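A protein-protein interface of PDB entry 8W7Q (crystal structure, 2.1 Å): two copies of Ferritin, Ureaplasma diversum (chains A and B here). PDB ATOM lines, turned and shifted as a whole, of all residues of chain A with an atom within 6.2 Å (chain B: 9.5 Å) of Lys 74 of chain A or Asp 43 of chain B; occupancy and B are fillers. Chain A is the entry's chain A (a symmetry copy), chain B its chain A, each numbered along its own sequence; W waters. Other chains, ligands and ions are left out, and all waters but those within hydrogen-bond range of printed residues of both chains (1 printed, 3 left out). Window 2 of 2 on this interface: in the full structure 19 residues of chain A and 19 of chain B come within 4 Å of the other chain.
The side-chain hydroxyl (OG) of Ser 70 of chain A is in hydrogen-bond range of a ring nitrogen (ND1) of His 39 of chain B, 2.9 Å away. NZ of Lys 74 of chain A lies within hydrogen-bond range of ND1 of His 39 of chain B (3.3 Å). The side-chain amide nitrogen (NE2) of Gln 55 of chain B sits at hydrogen-bond distance from the side-chain carboxylate (OE1) of Glu 67 of chain A, at 3.3 Å.
No position is printed for both chains. Of the 6 pairs that touch across the chains among the printed residues, none has its exchanged pair printed and touching as well.
Of the 23 printed residues of chain B, 4 touch a printed residue of chain A. Of the 11 printed residues of chain A, 4 touch a printed residue of chain B. Hydrophobic or aromatic side chains of chain A that line the printed part of chain B: Phe 73. Among the printed residues, no Asp or Glu carboxylate lies within 4 Å of a Lys or Arg side-chain nitrogen of the other chain.
Among the printed residues, pairs that only touch across the chains: Lys 74 of chain A with Asp 42 of chain B, Lys 74 of chain A with Asp 43 of chain B and Phe 73 of chain A with His 39 of chain B.
Lys 74 of chain A touches just these residues of chain B: His 39, Asp 42 and Asp 43. Of chain A, only Lys 74 comes within 4 Å of Asp 43 of chain B. Printed residues of chain A within 4 Å of Gln 55 of chain B: Glu 67. Of the printed residues of chain B, Ser 70 of chain A touches His 39 (2.9 Å). Printed residues of chain B within 4 Å of Glu 67 of chain A: Gln 55. Of the printed residues of chain A, Asp 42 of chain B touches Lys 74. Printed residues of chain A within 4 Å of His 39 of chain B: Ser 70 (2.9 Å), Phe 73 (3.9 Å) and Lys 74 (3.3 Å). Asp 46 of chain B touches none of the printed residues of chain A. Ala 41 of chain B touches none of the printed residues of chain A. The nearest printed residue of chain B that does not touch Glu 67 of chain A is Ala 35 of chain B (4.4 Å).
Water W1 bridges OD1 of Asp 43 of chain B and O of Lys 74 of chain A.
The side-chain hydroxyl of Ser 70 of chain A lies within hydrogen-bond range of the side-chain amino group of Lys 74 of chain A, at 3.1 Å. The backbone carbonyl oxygen of Phe 73 of chain A sits close to the side-chain amide oxygen of Asn 76 of chain A, 3.2 Å away. The backbone NH (N) of Met 78 of chain A sits at hydrogen-bond distance from the backbone carbonyl oxygen (O) of Phe 73 of chain A (3.5 Å).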
ATOM      1  N   GLU A  67      -5.349  33.739  21.105  1.00  0.00           N
ATOM      2  CA  GLU A  67      -5.591  32.924  19.920  1.00  0.00           C
ATOM      3  C   GLU A  67      -4.465  33.051  18.898  1.00  0.00           C
ATOM      4  O   GLU A  67      -4.146  32.079  18.209  1.00  0.00           O
ATOM      5  CB  GLU A  67      -6.941  33.278  19.290  1.00  0.00           C
ATOM      6  CG  GLU A  67      -8.164  32.802  20.110  1.00  0.00           C
ATOM      7  CD  GLU A  67      -8.216  31.261  20.285  1.00  0.00           C
ATOM      8  OE1 GLU A  67      -8.483  30.790  21.418  1.00  0.00           O
ATOM      9  OE2 GLU A  67      -7.950  30.523  19.300  1.00  0.00           O
ATOM     10  N   ILE A  69      -1.366  33.190  19.522  1.00  0.00           N
ATOM     11  CA  ILE A  69      -0.305  32.284  19.960  1.00  0.00           C
ATOM     12  C   ILE A  69      -0.637  30.845  19.587  1.00  0.00           C
ATOM     13  O   ILE A  69       0.202  30.121  19.041  1.00  0.00           O
ATOM     14  CB  ILE A  69      -0.059  32.441  21.470  1.00  0.00           C
ATOM     15  CG1 ILE A  69       0.647  33.779  21.735  1.00  0.00           C
ATOM     16  CG2 ILE A  69       0.749  31.264  22.009  1.00  0.00           C
ATOM     17  CD1 ILE A  69       0.573  34.246  23.169  1.00  0.00           C
ATOM     18  N   SER A  70      -1.868  30.412  19.860  1.00  0.00           N
ATOM     19  CA  SER A  70      -2.245  29.045  19.524  1.00  0.00           C
ATOM     20  C   SER A  70      -2.157  28.812  18.016  1.00  0.00           C
ATOM     21  O   SER A  70      -1.702  27.751  17.562  1.00  0.00           O
ATOM     22  CB  SER A  70      -3.658  28.756  20.048  1.00  0.00           C
ATOM     23  OG  SER A  70      -4.267  27.719  19.292  1.00  0.00           O
ATOM     24  N   ASP A  71      -2.558  29.813  17.225  1.00  0.00           N
ATOM     25  CA  ASP A  71      -2.453  29.730  15.770  1.00  0.00           C
ATOM     26  C   ASP A  71      -1.004  29.656  15.305  1.00  0.00           C
ATOM     27  O   ASP A  71      -0.682  28.888  14.392  1.00  0.00           O
ATOM     28  CB  ASP A  71      -3.137  30.937  15.126  1.00  0.00           C
ATOM     29  CG  ASP A  71      -2.946  30.973  13.623  1.00  0.00           C
ATOM     30  OD1 ASP A  71      -3.674  30.215  12.931  1.00  0.00           O
ATOM     31  OD2 ASP A  71      -2.070  31.740  13.137  1.00  0.00           O
ATOM     32  N   TYR A  72      -0.135  30.496  15.871  1.00  0.00           N
ATOM     33  CA  TYR A  72       1.292  30.418  15.583  1.00  0.00           C
ATOM     34  C   TYR A  72       1.832  29.018  15.851  1.00  0.00           C
ATOM     35  O   TYR A  72       2.548  28.442  15.021  1.00  0.00           O
ATOM     36  CB  TYR A  72       2.037  31.455  16.434  1.00  0.00           C
ATOM     37  CG  TYR A  72       3.516  31.553  16.135  1.00  0.00           C
ATOM     38  CD1 TYR A  72       3.975  31.593  14.822  1.00  0.00           C
ATOM     39  CD2 TYR A  72       4.451  31.645  17.159  1.00  0.00           C
ATOM     40  CE1 TYR A  72       5.327  31.698  14.537  1.00  0.00           C
ATOM     41  CE2 TYR A  72       5.813  31.749  16.885  1.00  0.00           C
ATOM     42  CZ  TYR A  72       6.244  31.775  15.569  1.00  0.00           C
ATOM     43  OH  TYR A  72       7.595  31.874  15.275  1.00  0.00           O
ATOM     44  N   PHE A  73       1.479  28.450  17.012  1.00  0.00           N
ATOM     45  CA  PHE A  73       1.961  27.116  17.374  1.00  0.00           C
ATOM     46  C   PHE A  73       1.540  26.070  16.339  1.00  0.00           C
ATOM     47  O   PHE A  73       2.322  25.168  16.009  1.00  0.00           O
ATOM     48  CB  PHE A  73       1.455  26.736  18.764  1.00  0.00           C
ATOM     49  CG  PHE A  73       2.154  27.448  19.897  1.00  0.00           C
ATOM     50  CD1 PHE A  73       3.174  28.350  19.657  1.00  0.00           C
ATOM     51  CD2 PHE A  73       1.792  27.190  21.213  1.00  0.00           C
ATOM     52  CE1 PHE A  73       3.815  28.988  20.701  1.00  0.00           C
ATOM     53  CE2 PHE A  73       2.431  27.818  22.267  1.00  0.00           C
ATOM     54  CZ  PHE A  73       3.442  28.725  22.010  1.00  0.00           C
ATOM     55  N   LYS A  74       0.311  26.185  15.809  1.00  0.00           N
ATOM     56  CA  LYS A  74      -0.154  25.304  14.737  1.00  0.00           C
ATOM     57  C   LYS A  74       0.768  25.345  13.531  1.00  0.00           C
ATOM     58  O   LYS A  74       0.919  24.340  12.826  1.00  0.00           O
ATOM     59  CB  LYS A  74      -1.554  25.715  14.254  1.00  0.00           C
ATOM     60  CG  LYS A  74      -2.733  25.368  15.136  1.00  0.00           C
ATOM     61  CD  LYS A  74      -4.027  25.795  14.405  1.00  0.00           C
ATOM     62  CE  LYS A  74      -5.250  25.820  15.319  1.00  0.00           C
ATOM     63  NZ  LYS A  74      -5.027  26.643  16.541  1.00  0.00           N
ATOM     64  N   ARG A  75       1.351  26.502  13.249  1.00  0.00           N
ATOM     65  CA  ARG A  75       2.089  26.672  12.005  1.00  0.00           C
ATOM     66  C   ARG A  75       3.521  26.160  12.089  1.00  0.00           C
ATOM     67  O   ARG A  75       4.107  25.818  11.057  1.00  0.00           O
ATOM     68  CB  ARG A  75       2.088  28.147  11.609  1.00  0.00           C
ATOM     69  CG  ARG A  75       0.685  28.723  11.329  1.00  0.00           C
ATOM     70  CD  ARG A  75       0.795  30.235  11.120  1.00  0.00           C
ATOM     71  NE  ARG A  75      -0.488  30.908  10.983  1.00  0.00           N
ATOM     72  CZ  ARG A  75      -1.036  31.240   9.815  1.00  0.00           C
ATOM     73  NH1 ARG A  75      -0.420  30.938   8.681  1.00  0.00           N
ATOM     74  NH2 ARG A  75      -2.199  31.883   9.778  1.00  0.00           N
ATOM     75  N   ASN A  76       4.114  26.110  13.280  1.00  0.00           N
ATOM     76  CA  ASN A  76       5.548  25.870  13.364  1.00  0.00           C
ATOM     77  C   ASN A  76       5.937  24.667  14.210  1.00  0.00           C
ATOM     78  O   ASN A  76       7.130  24.466  14.440  1.00  0.00           O
ATOM     79  CB  ASN A  76       6.266  27.120  13.898  1.00  0.00           C
ATOM     80  CG  ASN A  76       5.842  27.486  15.299  1.00  0.00           C
ATOM     81  OD1 ASN A  76       5.060  26.783  15.947  1.00  0.00           O
ATOM     82  ND2 ASN A  76       6.363  28.593  15.784  1.00  0.00           N
ATOM     83  N   GLY A  77       4.981  23.876  14.687  1.00  0.00           N
ATOM     84  CA  GLY A  77       5.290  22.719  15.496  1.00  0.00           C
ATOM     85  C   GLY A  77       5.459  22.977  16.980  1.00  0.00           C
ATOM     86  O   GLY A  77       5.729  22.030  17.729  1.00  0.00           O
ATOM     87  N   MET A  78       5.313  24.213  17.441  1.00  0.00           N
ATOM     88  CA  MET A  78       5.407  24.406  18.875  1.00  0.00           C
ATOM     89  C   MET A  78       4.207  23.777  19.575  1.00  0.00           C
ATOM     90  O   MET A  78       3.145  23.569  18.982  1.00  0.00           O
ATOM     91  CB  MET A  78       5.520  25.884  19.213  1.00  0.00           C
ATOM     92  CG  MET A  78       6.859  26.458  18.847  1.00  0.00           C
ATOM     93  SD  MET A  78       6.938  28.204  19.236  1.00  0.00           S
ATOM     94  CE  MET A  78       8.599  28.573  18.659  1.00  0.00           C
ATOM     95  N   TYR B  34     -11.901  23.616  26.177  1.00  0.00           N
ATOM     96  CA  TYR B  34     -12.361  23.559  24.797  1.00  0.00           C
ATOM     97  C   TYR B  34     -11.411  24.315  23.874  1.00  0.00           C
ATOM     98  O   TYR B  34     -11.135  23.859  22.759  1.00  0.00           O
ATOM     99  CB  TYR B  34     -13.785  24.106  24.694  1.00  0.00           C
ATOM    100  CG  TYR B  34     -14.854  23.196  25.276  1.00  0.00           C
ATOM    101  CD1 TYR B  34     -14.569  21.892  25.661  1.00  0.00           C
ATOM    102  CD2 TYR B  34     -16.152  23.647  25.437  1.00  0.00           C
ATOM    103  CE1 TYR B  34     -15.556  21.071  26.193  1.00  0.00           C
ATOM    104  CE2 TYR B  34     -17.135  22.840  25.969  1.00  0.00           C
ATOM    105  CZ  TYR B  34     -16.839  21.555  26.339  1.00  0.00           C
ATOM    106  OH  TYR B  34     -17.845  20.768  26.861  1.00  0.00           O
ATOM    107  N   ALA B  35     -10.869  25.456  24.331  1.00  0.00           N
ATOM    108  CA  ALA B  35      -9.916  26.181  23.488  1.00  0.00           C
ATOM    109  C   ALA B  35      -8.696  25.321  23.201  1.00  0.00           C
ATOM    110  O   ALA B  35      -8.151  25.353  22.095  1.00  0.00           O
ATOM    111  CB  ALA B  35      -9.482  27.496  24.137  1.00  0.00           C
ATOM    112  N   HIS B  36      -8.257  24.538  24.186  1.00  0.00           N
ATOM    113  CA  HIS B  36      -7.145  23.627  23.947  1.00  0.00           C
ATOM    114  C   HIS B  36      -7.559  22.526  22.983  1.00  0.00           C
ATOM    115  O   HIS B  36      -6.849  22.238  22.013  1.00  0.00           O
ATOM    116  CB  HIS B  36      -6.659  23.025  25.266  1.00  0.00           C
ATOM    117  CG  HIS B  36      -5.296  22.434  25.179  1.00  0.00           C
ATOM    118  ND1 HIS B  36      -4.189  23.033  25.742  1.00  0.00           N
ATOM    119  CD2 HIS B  36      -4.850  21.306  24.574  1.00  0.00           C
ATOM    120  CE1 HIS B  36      -3.118  22.299  25.486  1.00  0.00           C
ATOM    121  NE2 HIS B  36      -3.493  21.246  24.780  1.00  0.00           N
ATOM    122  N   TYR B  37      -8.720  21.915  23.230  1.00  0.00           N
ATOM    123  CA  TYR B  37      -9.221  20.869  22.346  1.00  0.00           C
ATOM    124  C   TYR B  37      -9.372  21.368  20.913  1.00  0.00           C
ATOM    125  O   TYR B  37      -9.146  20.607  19.969  1.00  0.00           O
ATOM    126  CB  TYR B  37     -10.557  20.339  22.860  1.00  0.00           C
ATOM    127  CG  TYR B  37     -10.468  19.436  24.073  1.00  0.00           C
ATOM    128  CD1 TYR B  37      -9.248  19.181  24.702  1.00  0.00           C
ATOM    129  CD2 TYR B  37     -11.611  18.830  24.593  1.00  0.00           C
ATOM    130  CE1 TYR B  37      -9.173  18.351  25.814  1.00  0.00           C
ATOM    131  CE2 TYR B  37     -11.544  18.002  25.692  1.00  0.00           C
ATOM    132  CZ  TYR B  37     -10.324  17.767  26.301  1.00  0.00           C
ATOM    133  OH  TYR B  37     -10.267  16.946  27.401  1.00  0.00           O
ATOM    134  N   ALA B  38      -9.761  22.636  20.728  1.00  0.00           N
ATOM    135  CA  ALA B  38      -9.907  23.176  19.376  1.00  0.00           C
ATOM    136  C   ALA B  38      -8.562  23.227  18.669  1.00  0.00           C
ATOM    137  O   ALA B  38      -8.444  22.862  17.492  1.00  0.00           O
ATOM    138  CB  ALA B  38     -10.524  24.580  19.414  1.00  0.00           C
ATOM    139  N   HIS B  39      -7.542  23.718  19.371  1.00  0.00           N
ATOM    140  CA  HIS B  39      -6.180  23.687  18.861  1.00  0.00           C
ATOM    141  C   HIS B  39      -5.781  22.272  18.457  1.00  0.00           C
ATOM    142  O   HIS B  39      -5.282  22.040  17.352  1.00  0.00           O
ATOM    143  CB  HIS B  39      -5.226  24.223  19.928  1.00  0.00           C
ATOM    144  CG  HIS B  39      -3.784  24.133  19.537  1.00  0.00           C
ATOM    145  ND1 HIS B  39      -3.159  25.093  18.774  1.00  0.00           N
ATOM    146  CD2 HIS B  39      -2.854  23.183  19.785  1.00  0.00           C
ATOM    147  CE1 HIS B  39      -1.896  24.750  18.587  1.00  0.00           C
ATOM    148  NE2 HIS B  39      -1.689  23.592  19.183  1.00  0.00           N
ATOM    149  N   VAL B  40      -6.039  21.306  19.336  1.00  0.00           N
ATOM    150  CA  VAL B  40      -5.619  19.932  19.093  1.00  0.00           C
ATOM    151  C   VAL B  40      -6.362  19.322  17.902  1.00  0.00           C
ATOM    152  O   VAL B  40      -5.758  18.628  17.078  1.00  0.00           O
ATOM    153  CB  VAL B  40      -5.806  19.106  20.380  1.00  0.00           C
ATOM    154  CG1 VAL B  40      -5.657  17.633  20.093  1.00  0.00           C
ATOM    155  CG2 VAL B  40      -4.785  19.539  21.430  1.00  0.00           C
ATOM    156  N   ALA B  41      -7.682  19.531  17.804  1.00  0.00           N
ATOM    157  CA  ALA B  41      -8.432  18.993  16.670  1.00  0.00           C
ATOM    158  C   ALA B  41      -7.806  19.418  15.346  1.00  0.00           C
ATOM    159  O   ALA B  41      -7.638  18.613  14.424  1.00  0.00           O
ATOM    160  CB  ALA B  41      -9.892  19.460  16.721  1.00  0.00           C
ATOM    161  N   ASP B  42      -7.486  20.700  15.228  1.00  0.00           N
ATOM    162  CA  ASP B  42      -6.861  21.198  14.015  1.00  0.00           C
ATOM    163  C   ASP B  42      -5.427  20.709  13.922  1.00  0.00           C
ATOM    164  O   ASP B  42      -5.041  20.034  12.957  1.00  0.00           O
ATOM    165  CB  ASP B  42      -6.938  22.731  13.999  1.00  0.00           C
ATOM    166  CG  ASP B  42      -6.488  23.336  12.681  1.00  0.00           C
ATOM    167  OD1 ASP B  42      -6.036  22.590  11.800  1.00  0.00           O
ATOM    168  OD2 ASP B  42      -6.598  24.568  12.531  1.00  0.00           O
ATOM    169  N   ASP B  43      -4.638  20.988  14.952  1.00  0.00           N
ATOM    170  CA  ASP B  43      -3.194  20.862  14.829  1.00  0.00           C
ATOM    171  C   ASP B  43      -2.764  19.405  14.769  1.00  0.00           C
ATOM    172  O   ASP B  43      -1.960  19.023  13.911  1.00  0.00           O
ATOM    173  CB  ASP B  43      -2.514  21.585  15.979  1.00  0.00           C
ATOM    174  CG  ASP B  43      -1.014  21.412  15.962  1.00  0.00           C
ATOM    175  OD1 ASP B  43      -0.402  21.738  14.924  1.00  0.00           O
ATOM    176  OD2 ASP B  43      -0.447  20.998  17.000  1.00  0.00           O
ATOM    177  N   GLU B  44      -3.288  18.567  15.660  1.00  0.00           N
ATOM    178  CA  GLU B  44      -2.842  17.184  15.658  1.00  0.00           C
ATOM    179  C   GLU B  44      -3.761  16.237  14.904  1.00  0.00           C
ATOM    180  O   GLU B  44      -3.275  15.271  14.322  1.00  0.00           O
ATOM    181  CB  GLU B  44      -2.635  16.685  17.087  1.00  0.00           C
ATOM    182  CG  GLU B  44      -1.143  16.639  17.416  1.00  0.00           C
ATOM    183  CD  GLU B  44      -0.820  16.997  18.855  1.00  0.00           C
ATOM    184  OE1 GLU B  44       0.176  17.733  19.069  1.00  0.00           O
ATOM    185  OE2 GLU B  44      -1.531  16.517  19.768  1.00  0.00           O
ATOM    186  N   PHE B  45      -5.065  16.477  14.863  1.00  0.00           N
ATOM    187  CA  PHE B  45      -5.944  15.541  14.173  1.00  0.00           C
ATOM    188  C   PHE B  45      -6.294  15.961  12.749  1.00  0.00           C
ATOM    189  O   PHE B  45      -7.005  15.230  12.059  1.00  0.00           O
ATOM    190  CB  PHE B  45      -7.208  15.321  15.002  1.00  0.00           C
ATOM    191  CG  PHE B  45      -6.932  14.769  16.381  1.00  0.00           C
ATOM    192  CD1 PHE B  45      -5.843  13.941  16.612  1.00  0.00           C
ATOM    193  CD2 PHE B  45      -7.768  15.076  17.439  1.00  0.00           C
ATOM    194  CE1 PHE B  45      -5.591  13.436  17.871  1.00  0.00           C
ATOM    195  CE2 PHE B  45      -7.523  14.571  18.699  1.00  0.00           C
ATOM    196  CZ  PHE B  45      -6.430  13.753  18.919  1.00  0.00           C
ATOM    197  N   ASP B  46      -5.784  17.101  12.292  1.00  0.00           N
ATOM    198  CA  ASP B  46      -5.999  17.596  10.934  1.00  0.00           C
ATOM    199  C   ASP B  46      -7.477  17.755  10.606  1.00  0.00           C
ATOM    200  O   ASP B  46      -7.932  17.416   9.508  1.00  0.00           O
ATOM    201  CB  ASP B  46      -5.303  16.716   9.891  1.00  0.00           C
ATOM    202  CG  ASP B  46      -3.853  16.407  10.262  1.00  0.00           C
ATOM    203  OD1 ASP B  46      -3.097  17.357  10.481  1.00  0.00           O
ATOM    204  OD2 ASP B  46      -3.538  15.217  10.460  1.00  0.00           O
ATOM    205  N   MET B  47      -8.223  18.317  11.546  1.00  0.00           N
ATOM    206  CA  MET B  47      -9.653  18.543  11.378  1.00  0.00           C
ATOM    207  C   MET B  47      -9.949  19.984  11.738  1.00  0.00           C
ATOM    208  O   MET B  47     -10.482  20.271  12.818  1.00  0.00           O
ATOM    209  CB  MET B  47     -10.449  17.562  12.228  1.00  0.00           C
ATOM    210  CG  MET B  47     -10.261  16.127  11.785  1.00  0.00           C
ATOM    211  SD  MET B  47     -11.419  14.991  12.557  1.00  0.00           S
ATOM    212  CE  MET B  47     -12.888  15.242  11.541  1.00  0.00           C
ATOM    213  N   PRO B  48      -9.608  20.926  10.859  1.00  0.00           N
ATOM    214  CA  PRO B  48      -9.838  22.343  11.171  1.00  0.00           C
ATOM    215  C   PRO B  48     -11.296  22.697  11.429  1.00  0.00           C
ATOM    216  O   PRO B  48     -11.562  23.579  12.253  1.00  0.00           O
ATOM    217  CB  PRO B  48      -9.280  23.069   9.935  1.00  0.00           C
ATOM    218  CG  PRO B  48      -9.160  22.022   8.875  1.00  0.00           C
ATOM    219  CD  PRO B  48      -8.854  20.754   9.607  1.00  0.00           C
ATOM    220  N   TYR B  49     -12.256  22.058  10.754  1.00  0.00           N
ATOM    221  CA  TYR B  49     -13.647  22.426  11.000  1.00  0.00           C
ATOM    222  C   TYR B  49     -14.146  21.877  12.331  1.00  0.00           C
ATOM    223  O   TYR B  49     -14.911  22.552  13.032  1.00  0.00           O
ATOM    224  CB  TYR B  49     -14.521  21.979   9.835  1.00  0.00           C
ATOM    225  CG  TYR B  49     -14.269  22.842   8.629  1.00  0.00           C
ATOM    226  CD1 TYR B  49     -14.681  24.167   8.608  1.00  0.00           C
ATOM    227  CD2 TYR B  49     -13.568  22.352   7.536  1.00  0.00           C
ATOM    228  CE1 TYR B  49     -14.425  24.978   7.516  1.00  0.00           C
ATOM    229  CE2 TYR B  49     -13.310  23.154   6.436  1.00  0.00           C
ATOM    230  CZ  TYR B  49     -13.742  24.463   6.435  1.00  0.00           C
ATOM    231  OH  TYR B  49     -13.489  25.256   5.346  1.00  0.00           O
ATOM    232  N   LEU B  50     -13.712  20.681  12.717  1.00  0.00           N
ATOM    233  CA  LEU B  50     -13.938  20.253  14.089  1.00  0.00           C
ATOM    234  C   LEU B  50     -13.346  21.265  15.070  1.00  0.00           C
ATOM    235  O   LEU B  50     -13.989  21.631  16.064  1.00  0.00           O
ATOM    236  CB  LEU B  50     -13.340  18.866  14.299  1.00  0.00           C
ATOM    237  CG  LEU B  50     -13.457  18.300  15.715  1.00  0.00           C
ATOM    238  CD1 LEU B  50     -14.915  18.115  16.093  1.00  0.00           C
ATOM    239  CD2 LEU B  50     -12.709  16.991  15.805  1.00  0.00           C
ATOM    240  N   GLY B  51     -12.141  21.764  14.776  1.00  0.00           N
ATOM    241  CA  GLY B  51     -11.536  22.772  15.638  1.00  0.00           C
ATOM    242  C   GLY B  51     -12.401  24.007  15.771  1.00  0.00           C
ATOM    243  O   GLY B  51     -12.596  24.536  16.868  1.00  0.00           O
ATOM    244  N   LYS B  52     -12.953  24.472  14.650  1.00  0.00           N
ATOM    245  CA  LYS B  52     -13.787  25.662  14.683  1.00  0.00           C
ATOM    246  C   LYS B  52     -15.070  25.401  15.456  1.00  0.00           C
ATOM    247  O   LYS B  52     -15.536  26.262  16.204  1.00  0.00           O
ATOM    248  CB  LYS B  52     -14.112  26.109  13.259  1.00  0.00           C
ATOM    249  CG  LYS B  52     -13.140  27.118  12.711  1.00  0.00           C
ATOM    250  CD  LYS B  52     -12.720  26.735  11.312  1.00  0.00           C
ATOM    251  CE  LYS B  52     -13.500  27.549  10.305  1.00  0.00           C
ATOM    252  NZ  LYS B  52     -12.654  27.932   9.144  1.00  0.00           N
ATOM    253  N   GLN B  55     -14.050  25.492  18.990  1.00  0.00           N
ATOM    254  CA  GLN B  55     -13.714  26.864  19.362  1.00  0.00           C
ATOM    255  C   GLN B  55     -14.937  27.740  19.605  1.00  0.00           C
ATOM    256  O   GLN B  55     -14.943  28.550  20.489  1.00  0.00           O
ATOM    257  CB  GLN B  55     -12.768  27.503  18.355  1.00  0.00           C
ATOM    258  CG  GLN B  55     -12.314  28.915  18.648  1.00  0.00           C
ATOM    259  CD  GLN B  55     -11.353  28.990  19.807  1.00  0.00           C
ATOM    260  OE1 GLN B  55     -10.433  28.203  19.902  1.00  0.00           O
ATOM    261  NE2 GLN B  55     -11.565  29.941  20.694  1.00  0.00           N
ATOM    262  N   LEU B  98     -12.063  12.813  21.242  1.00  0.00           N
ATOM    263  CA  LEU B  98     -12.074  14.221  21.618  1.00  0.00           C
ATOM    264  C   LEU B  98     -13.489  14.781  21.738  1.00  0.00           C
ATOM    265  O   LEU B  98     -13.823  15.366  22.729  1.00  0.00           O
ATOM    266  CB  LEU B  98     -11.249  15.042  20.647  1.00  0.00           C
ATOM    267  CG  LEU B  98     -10.855  16.465  21.010  1.00  0.00           C
ATOM    268  CD1 LEU B  98      -9.669  16.451  21.947  1.00  0.00           C
ATOM    269  CD2 LEU B  98     -10.501  17.216  19.748  1.00  0.00           C
ATOM    270  N   LYS B 159     -12.126  10.977   7.251  1.00  0.00           N
ATOM    271  CA  LYS B 159     -11.999  12.226   7.990  1.00  0.00           C
ATOM    272  C   LYS B 159     -12.437  13.429   7.162  1.00  0.00           C
ATOM    273  O   LYS B 159     -13.079  14.351   7.686  1.00  0.00           O
ATOM    274  CB  LYS B 159     -10.547  12.401   8.426  1.00  0.00           C
ATOM    275  CG  LYS B 159     -10.306  12.459   9.896  1.00  0.00           C
ATOM    276  CD  LYS B 159      -8.880  12.932  10.151  1.00  0.00           C
ATOM    277  CE  LYS B 159      -8.355  12.345  11.432  1.00  0.00           C
ATOM    278  NZ  LYS B 159      -6.947  12.724  11.637  1.00  0.00           N
ATOM    279  N   GLU B 163     -15.261  16.121   7.930  1.00  0.00           N
ATOM    280  CA  GLU B 163     -14.911  17.539   7.969  1.00  0.00           C
ATOM    281  C   GLU B 163     -15.857  18.374   7.113  1.00  0.00           C
ATOM    282  O   GLU B 163     -16.271  19.470   7.515  1.00  0.00           O
ATOM    283  CB  GLU B 163     -13.466  17.722   7.497  1.00  0.00           C
ATOM    284  CG  GLU B 163     -12.456  17.563   8.611  1.00  0.00           C
ATOM    285  CD  GLU B 163     -12.397  18.799   9.503  1.00  0.00           C
ATOM    286  OE1 GLU B 163     -11.825  19.828   9.079  1.00  0.00           O
ATOM    287  OE2 GLU B 163     -12.931  18.742  10.629  1.00  0.00           O
HETATM  288  O   HOH W   1      -0.537  21.870  12.497  1.00  0.00           O
